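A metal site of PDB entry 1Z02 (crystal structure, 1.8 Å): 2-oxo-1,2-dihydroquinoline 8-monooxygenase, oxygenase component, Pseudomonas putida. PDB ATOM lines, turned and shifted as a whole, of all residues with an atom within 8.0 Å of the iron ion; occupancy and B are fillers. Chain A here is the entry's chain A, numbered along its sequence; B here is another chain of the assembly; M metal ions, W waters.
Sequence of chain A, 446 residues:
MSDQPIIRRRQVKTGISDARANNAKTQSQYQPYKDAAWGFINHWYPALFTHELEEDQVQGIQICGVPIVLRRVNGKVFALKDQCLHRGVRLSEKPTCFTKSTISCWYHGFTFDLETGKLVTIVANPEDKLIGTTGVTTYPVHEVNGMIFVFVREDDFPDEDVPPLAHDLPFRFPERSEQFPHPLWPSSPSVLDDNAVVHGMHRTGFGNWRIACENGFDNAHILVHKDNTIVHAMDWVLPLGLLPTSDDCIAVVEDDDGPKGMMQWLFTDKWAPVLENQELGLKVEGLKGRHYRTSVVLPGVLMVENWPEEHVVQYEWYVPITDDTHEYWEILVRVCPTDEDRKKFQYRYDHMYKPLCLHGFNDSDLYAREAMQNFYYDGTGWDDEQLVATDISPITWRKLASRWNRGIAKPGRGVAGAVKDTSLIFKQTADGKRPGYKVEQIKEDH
The side-chain carboxylate (OD1) of Asp 365 lies close to the side-chain amide nitrogen (ND2) of Asn 362. A ring nitrogen (ND1) of His 225 lies within hydrogen-bond range of the side-chain amide nitrogen (ND2) of Asn 228, 2.9 Å away. A ring nitrogen (ND1) of His 225 is in hydrogen-bond range of the backbone carbonyl oxygen (O) of Phe 361 (3.1 Å). The side-chain carboxylate of Asp 365 sits close to the side-chain amide nitrogen of Asn 215, 3.2 Å away. The side-chain carboxylate of Asp 218 lies within hydrogen-bond range of a ring nitrogen (ND1) of His 221 (2.7 Å).
Of the 22 residues printed, 3 come within 4 Å of the iron ion.
The iron ion is bound by NE2 of His 225, NE2 of His 221, OD2 of Asp 365, water W1, water W2 and OD1 of Asp 365.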
ATOM      1  N   ASN A 215      19.946  26.030  21.987  1.00  0.00           N
ATOM      2  CA  ASN A 215      19.604  26.057  20.570  1.00  0.00           C
ATOM      3  C   ASN A 215      18.258  26.742  20.409  1.00  0.00           C
ATOM      4  O   ASN A 215      18.036  27.478  19.455  1.00  0.00           O
ATOM      5  CB  ASN A 215      19.540  24.626  20.014  1.00  0.00           C
ATOM      6  CG  ASN A 215      18.602  24.493  18.824  1.00  0.00           C
ATOM      7  OD1 ASN A 215      17.398  24.281  18.984  1.00  0.00           O
ATOM      8  ND2 ASN A 215      19.157  24.626  17.608  1.00  0.00           N
ATOM      9  N   GLY A 216      17.372  26.512  21.375  1.00  0.00           N
ATOM     10  CA  GLY A 216      16.035  27.092  21.339  1.00  0.00           C
ATOM     11  C   GLY A 216      15.977  28.589  21.101  1.00  0.00           C
ATOM     12  O   GLY A 216      15.133  29.054  20.339  1.00  0.00           O
ATOM     13  N   PHE A 217      16.872  29.342  21.744  1.00  0.00           N
ATOM     14  CA  PHE A 217      16.874  30.792  21.579  1.00  0.00           C
ATOM     15  C   PHE A 217      18.082  31.328  20.834  1.00  0.00           C
ATOM     16  O   PHE A 217      18.424  32.510  20.949  1.00  0.00           O
ATOM     17  CB  PHE A 217      16.718  31.492  22.944  1.00  0.00           C
ATOM     18  CG  PHE A 217      17.861  31.254  23.901  1.00  0.00           C
ATOM     19  CD1 PHE A 217      18.964  32.104  23.930  1.00  0.00           C
ATOM     20  CD2 PHE A 217      17.809  30.186  24.798  1.00  0.00           C
ATOM     21  CE1 PHE A 217      19.998  31.903  24.825  1.00  0.00           C
ATOM     22  CE2 PHE A 217      18.830  29.963  25.711  1.00  0.00           C
ATOM     23  CZ  PHE A 217      19.931  30.835  25.739  1.00  0.00           C
ATOM     24  N   ASP A 218      18.733  30.463  20.051  1.00  0.00           N
ATOM     25  CA  ASP A 218      19.891  30.851  19.257  1.00  0.00           C
ATOM     26  C   ASP A 218      19.404  31.797  18.144  1.00  0.00           C
ATOM     27  O   ASP A 218      18.442  31.491  17.436  1.00  0.00           O
ATOM     28  CB  ASP A 218      20.545  29.616  18.637  1.00  0.00           C
ATOM     29  CG  ASP A 218      21.781  29.964  17.850  1.00  0.00           C
ATOM     30  OD1 ASP A 218      22.866  30.045  18.467  1.00  0.00           O
ATOM     31  OD2 ASP A 218      21.663  30.178  16.628  1.00  0.00           O
ATOM     32  N   ASN A 219      20.079  32.932  17.978  1.00  0.00           N
ATOM     33  CA  ASN A 219      19.682  33.911  16.971  1.00  0.00           C
ATOM     34  C   ASN A 219      20.341  33.748  15.618  1.00  0.00           C
ATOM     35  O   ASN A 219      19.827  34.258  14.631  1.00  0.00           O
ATOM     36  CB  ASN A 219      19.942  35.324  17.468  1.00  0.00           C
ATOM     37  CG  ASN A 219      19.373  35.569  18.845  1.00  0.00           C
ATOM     38  OD1 ASN A 219      18.215  35.258  19.117  1.00  0.00           O
ATOM     39  ND2 ASN A 219      20.187  36.152  19.728  1.00  0.00           N
ATOM     40  N   ALA A 220      21.454  33.030  15.546  1.00  0.00           N
ATOM     41  CA  ALA A 220      22.148  32.921  14.270  1.00  0.00           C
ATOM     42  C   ALA A 220      22.396  31.508  13.715  1.00  0.00           C
ATOM     43  O   ALA A 220      23.506  30.991  13.841  1.00  0.00           O
ATOM     44  CB  ALA A 220      23.467  33.675  14.364  1.00  0.00           C
ATOM     45  N   HIS A 221      21.383  30.886  13.120  1.00  0.00           N
ATOM     46  CA  HIS A 221      21.574  29.553  12.530  1.00  0.00           C
ATOM     47  C   HIS A 221      20.664  29.332  11.333  1.00  0.00           C
ATOM     48  O   HIS A 221      19.831  28.417  11.303  1.00  0.00           O
ATOM     49  CB  HIS A 221      21.399  28.426  13.562  1.00  0.00           C
ATOM     50  CG  HIS A 221      20.042  28.370  14.213  1.00  0.00           C
ATOM     51  ND1 HIS A 221      19.598  29.337  15.097  1.00  0.00           N
ATOM     52  CD2 HIS A 221      19.078  27.437  14.154  1.00  0.00           C
ATOM     53  CE1 HIS A 221      18.412  28.983  15.562  1.00  0.00           C
ATOM     54  NE2 HIS A 221      18.072  27.841  15.005  1.00  0.00           N
ATOM     55  N   ILE A 222      20.843  30.183  10.325  1.00  0.00           N
ATOM     56  CA  ILE A 222      20.049  30.106   9.099  1.00  0.00           C
ATOM     57  C   ILE A 222      20.240  28.793   8.321  1.00  0.00           C
ATOM     58  O   ILE A 222      19.286  28.204   7.822  1.00  0.00           O
ATOM     59  CB  ILE A 222      20.382  31.287   8.153  1.00  0.00           C
ATOM     60  CG1 ILE A 222      19.601  31.167   6.838  1.00  0.00           C
ATOM     61  CG2 ILE A 222      21.896  31.354   7.874  1.00  0.00           C
ATOM     62  CD1 ILE A 222      19.861  32.314   5.841  1.00  0.00           C
ATOM     63  N   VAL A 224      20.490  25.966   9.181  1.00  0.00           N
ATOM     64  CA  VAL A 224      19.669  24.916   9.757  1.00  0.00           C
ATOM     65  C   VAL A 224      18.226  24.926   9.259  1.00  0.00           C
ATOM     66  O   VAL A 224      17.622  23.879   9.082  1.00  0.00           O
ATOM     67  CB  VAL A 224      19.674  25.005  11.312  1.00  0.00           C
ATOM     68  CG1 VAL A 224      18.657  24.029  11.911  1.00  0.00           C
ATOM     69  CG2 VAL A 224      21.084  24.739  11.863  1.00  0.00           C
ATOM     70  N   HIS A 225      17.674  26.112   9.018  1.00  0.00           N
ATOM     71  CA  HIS A 225      16.290  26.269   8.588  1.00  0.00           C
ATOM     72  C   HIS A 225      16.104  26.784   7.165  1.00  0.00           C
ATOM     73  O   HIS A 225      14.967  26.950   6.722  1.00  0.00           O
ATOM     74  CB  HIS A 225      15.552  27.235   9.540  1.00  0.00           C
ATOM     75  CG  HIS A 225      15.549  26.793  10.962  1.00  0.00           C
ATOM     76  ND1 HIS A 225      14.676  25.844  11.449  1.00  0.00           N
ATOM     77  CD2 HIS A 225      16.333  27.162  12.012  1.00  0.00           C
ATOM     78  CE1 HIS A 225      14.929  25.640  12.726  1.00  0.00           C
ATOM     79  NE2 HIS A 225      15.928  26.427  13.087  1.00  0.00           N
ATOM     80  N   ASN A 228      13.797  24.665   5.023  1.00  0.00           N
ATOM     81  CA  ASN A 228      12.467  24.372   5.543  1.00  0.00           C
ATOM     82  C   ASN A 228      11.385  24.813   4.552  1.00  0.00           C
ATOM     83  O   ASN A 228      11.464  25.886   3.935  1.00  0.00           O
ATOM     84  CB  ASN A 228      12.264  25.072   6.886  1.00  0.00           C
ATOM     85  CG  ASN A 228      13.143  24.498   7.976  1.00  0.00           C
ATOM     86  OD1 ASN A 228      13.867  23.518   7.772  1.00  0.00           O
ATOM     87  ND2 ASN A 228      13.082  25.110   9.145  1.00  0.00           N
ATOM     88  N   GLU A 316       8.565  26.852  24.666  1.00  0.00           N
ATOM     89  CA  GLU A 316       9.295  25.595  24.689  1.00  0.00           C
ATOM     90  C   GLU A 316       9.957  25.346  26.030  1.00  0.00           C
ATOM     91  O   GLU A 316      10.355  26.265  26.746  1.00  0.00           O
ATOM     92  CB  GLU A 316      10.373  25.558  23.602  1.00  0.00           C
ATOM     93  CG  GLU A 316       9.870  25.800  22.197  1.00  0.00           C
ATOM     94  CD  GLU A 316      10.928  25.471  21.151  1.00  0.00           C
ATOM     95  OE1 GLU A 316      12.127  25.613  21.456  1.00  0.00           O
ATOM     96  OE2 GLU A 316      10.543  25.087  20.034  1.00  0.00           O
ATOM     97  N   TYR A 328      11.462  17.512  25.219  1.00  0.00           N
ATOM     98  CA  TYR A 328      11.303  18.767  24.490  1.00  0.00           C
ATOM     99  C   TYR A 328       9.842  19.114  24.207  1.00  0.00           C
ATOM    100  O   TYR A 328       9.148  18.435  23.442  1.00  0.00           O
ATOM    101  CB  TYR A 328      12.115  18.665  23.197  1.00  0.00           C
ATOM    102  CG  TYR A 328      11.904  19.771  22.189  1.00  0.00           C
ATOM    103  CD1 TYR A 328      11.993  21.119  22.554  1.00  0.00           C
ATOM    104  CD2 TYR A 328      11.697  19.468  20.836  1.00  0.00           C
ATOM    105  CE1 TYR A 328      11.888  22.135  21.600  1.00  0.00           C
ATOM    106  CE2 TYR A 328      11.596  20.474  19.880  1.00  0.00           C
ATOM    107  CZ  TYR A 328      11.685  21.805  20.262  1.00  0.00           C
ATOM    108  OH  TYR A 328      11.619  22.777  19.283  1.00  0.00           O
ATOM    109  N   PHE A 361       9.551  23.230  10.694  1.00  0.00           N
ATOM    110  CA  PHE A 361      10.587  24.189  11.054  1.00  0.00           C
ATOM    111  C   PHE A 361      11.516  23.644  12.144  1.00  0.00           C
ATOM    112  O   PHE A 361      12.725  23.532  11.952  1.00  0.00           O
ATOM    113  CB  PHE A 361       9.937  25.495  11.537  1.00  0.00           C
ATOM    114  CG  PHE A 361      10.908  26.618  11.738  1.00  0.00           C
ATOM    115  CD1 PHE A 361      11.414  27.328  10.654  1.00  0.00           C
ATOM    116  CD2 PHE A 361      11.339  26.963  13.022  1.00  0.00           C
ATOM    117  CE1 PHE A 361      12.324  28.375  10.843  1.00  0.00           C
ATOM    118  CE2 PHE A 361      12.240  27.993  13.222  1.00  0.00           C
ATOM    119  CZ  PHE A 361      12.739  28.702  12.132  1.00  0.00           C
ATOM    120  N   ASN A 362      10.935  23.301  13.290  1.00  0.00           N
ATOM    121  CA  ASN A 362      11.703  22.821  14.438  1.00  0.00           C
ATOM    122  C   ASN A 362      12.322  21.417  14.407  1.00  0.00           C
ATOM    123  O   ASN A 362      13.203  21.131  15.213  1.00  0.00           O
ATOM    124  CB  ASN A 362      10.871  22.989  15.715  1.00  0.00           C
ATOM    125  CG  ASN A 362      10.641  24.447  16.057  1.00  0.00           C
ATOM    126  OD1 ASN A 362       9.510  24.938  16.083  1.00  0.00           O
ATOM    127  ND2 ASN A 362      11.724  25.162  16.296  1.00  0.00           N
ATOM    128  N   ASP A 363      11.884  20.541  13.517  1.00  0.00           N
ATOM    129  CA  ASP A 363      12.488  19.207  13.463  1.00  0.00           C
ATOM    130  C   ASP A 363      13.966  19.341  13.112  1.00  0.00           C
ATOM    131  O   ASP A 363      14.790  18.524  13.533  1.00  0.00           O
ATOM    132  CB  ASP A 363      11.799  18.333  12.419  1.00  0.00           C
ATOM    133  CG  ASP A 363      10.491  17.753  12.915  1.00  0.00           C
ATOM    134  OD1 ASP A 363       9.802  17.077  12.112  1.00  0.00           O
ATOM    135  OD2 ASP A 363      10.161  17.950  14.107  1.00  0.00           O
ATOM    136  N   SER A 364      14.321  20.369  12.343  1.00  0.00           N
ATOM    137  CA  SER A 364      15.707  20.594  11.951  1.00  0.00           C
ATOM    138  C   SER A 364      16.595  20.873  13.152  1.00  0.00           C
ATOM    139  O   SER A 364      17.785  20.543  13.148  1.00  0.00           O
ATOM    140  CB  SER A 364      15.799  21.764  10.965  1.00  0.00           C
ATOM    141  OG  SER A 364      15.082  21.478   9.779  1.00  0.00           O
ATOM    142  N   ASP A 365      16.027  21.498  14.175  1.00  0.00           N
ATOM    143  CA  ASP A 365      16.769  21.817  15.389  1.00  0.00           C
ATOM    144  C   ASP A 365      17.157  20.587  16.170  1.00  0.00           C
ATOM    145  O   ASP A 365      18.124  20.618  16.934  1.00  0.00           O
ATOM    146  CB  ASP A 365      15.936  22.748  16.271  1.00  0.00           C
ATOM    147  CG  ASP A 365      15.891  24.139  15.733  1.00  0.00           C
ATOM    148  OD1 ASP A 365      14.796  24.766  15.732  1.00  0.00           O
ATOM    149  OD2 ASP A 365      16.972  24.610  15.302  1.00  0.00           O
ATOM    150  N   LEU A 366      16.414  19.504  15.975  1.00  0.00           N
ATOM    151  CA  LEU A 366      16.669  18.234  16.656  1.00  0.00           C
ATOM    152  C   LEU A 366      18.003  17.648  16.245  1.00  0.00           C
ATOM    153  O   LEU A 366      18.787  17.210  17.090  1.00  0.00           O
ATOM    154  CB  LEU A 366      15.544  17.235  16.344  1.00  0.00           C
ATOM    155  CG  LEU A 366      14.501  16.974  17.422  1.00  0.00           C
ATOM    156  CD1 LEU A 366      14.129  18.256  18.123  1.00  0.00           C
ATOM    157  CD2 LEU A 366      13.298  16.308  16.807  1.00  0.00           C
ATOM    158  N   ALA A 368      20.439  19.306  14.976  1.00  0.00           N
ATOM    159  CA  ALA A 368      21.469  20.231  15.394  1.00  0.00           C
ATOM    160  C   ALA A 368      21.833  19.961  16.858  1.00  0.00           C
ATOM    161  O   ALA A 368      23.002  19.956  17.230  1.00  0.00           O
ATOM    162  CB  ALA A 368      20.991  21.680  15.222  1.00  0.00           C
ATOM    163  N   ARG A 369      20.819  19.731  17.680  1.00  0.00           N
ATOM    164  CA  ARG A 369      21.089  19.462  19.100  1.00  0.00           C
ATOM    165  C   ARG A 369      21.867  18.162  19.303  1.00  0.00           C
ATOM    166  O   ARG A 369      22.894  18.166  19.983  1.00  0.00           O
ATOM    167  CB  ARG A 369      19.774  19.427  19.869  1.00  0.00           C
ATOM    168  CG  ARG A 369      19.035  20.747  19.850  1.00  0.00           C
ATOM    169  CD  ARG A 369      17.592  20.573  20.288  1.00  0.00           C
ATOM    170  NE  ARG A 369      16.837  21.805  20.144  1.00  0.00           N
ATOM    171  CZ  ARG A 369      15.534  21.904  20.339  1.00  0.00           C
ATOM    172  NH1 ARG A 369      14.925  23.072  20.183  1.00  0.00           N
ATOM    173  NH2 ARG A 369      14.826  20.832  20.676  1.00  0.00           N
ATOM    174  N   TYR B 107      25.884  24.506  11.177  1.00  0.00           N
ATOM    175  CA  TYR B 107      25.123  25.104  12.259  1.00  0.00           C
ATOM    176  C   TYR B 107      25.207  26.632  12.223  1.00  0.00           C
ATOM    177  O   TYR B 107      24.222  27.292  11.917  1.00  0.00           O
ATOM    178  CB  TYR B 107      25.604  24.567  13.615  1.00  0.00           C
ATOM    179  CG  TYR B 107      24.667  24.888  14.752  1.00  0.00           C
ATOM    180  CD1 TYR B 107      24.941  24.480  16.057  1.00  0.00           C
ATOM    181  CD2 TYR B 107      23.493  25.613  14.538  1.00  0.00           C
ATOM    182  CE1 TYR B 107      24.087  24.794  17.112  1.00  0.00           C
ATOM    183  CE2 TYR B 107      22.631  25.926  15.586  1.00  0.00           C
ATOM    184  CZ  TYR B 107      22.929  25.514  16.864  1.00  0.00           C
ATOM    185  OH  TYR B 107      22.077  25.858  17.897  1.00  0.00           O
HETATM  186 FE    FE M   1      16.230  26.679  15.094  1.00  0.00          FE
HETATM  187  O   HOH W   1      15.713  26.563  17.290  1.00  0.00           O
HETATM  188  O   HOH W   2      14.983  28.453  15.937  1.00  0.00           O
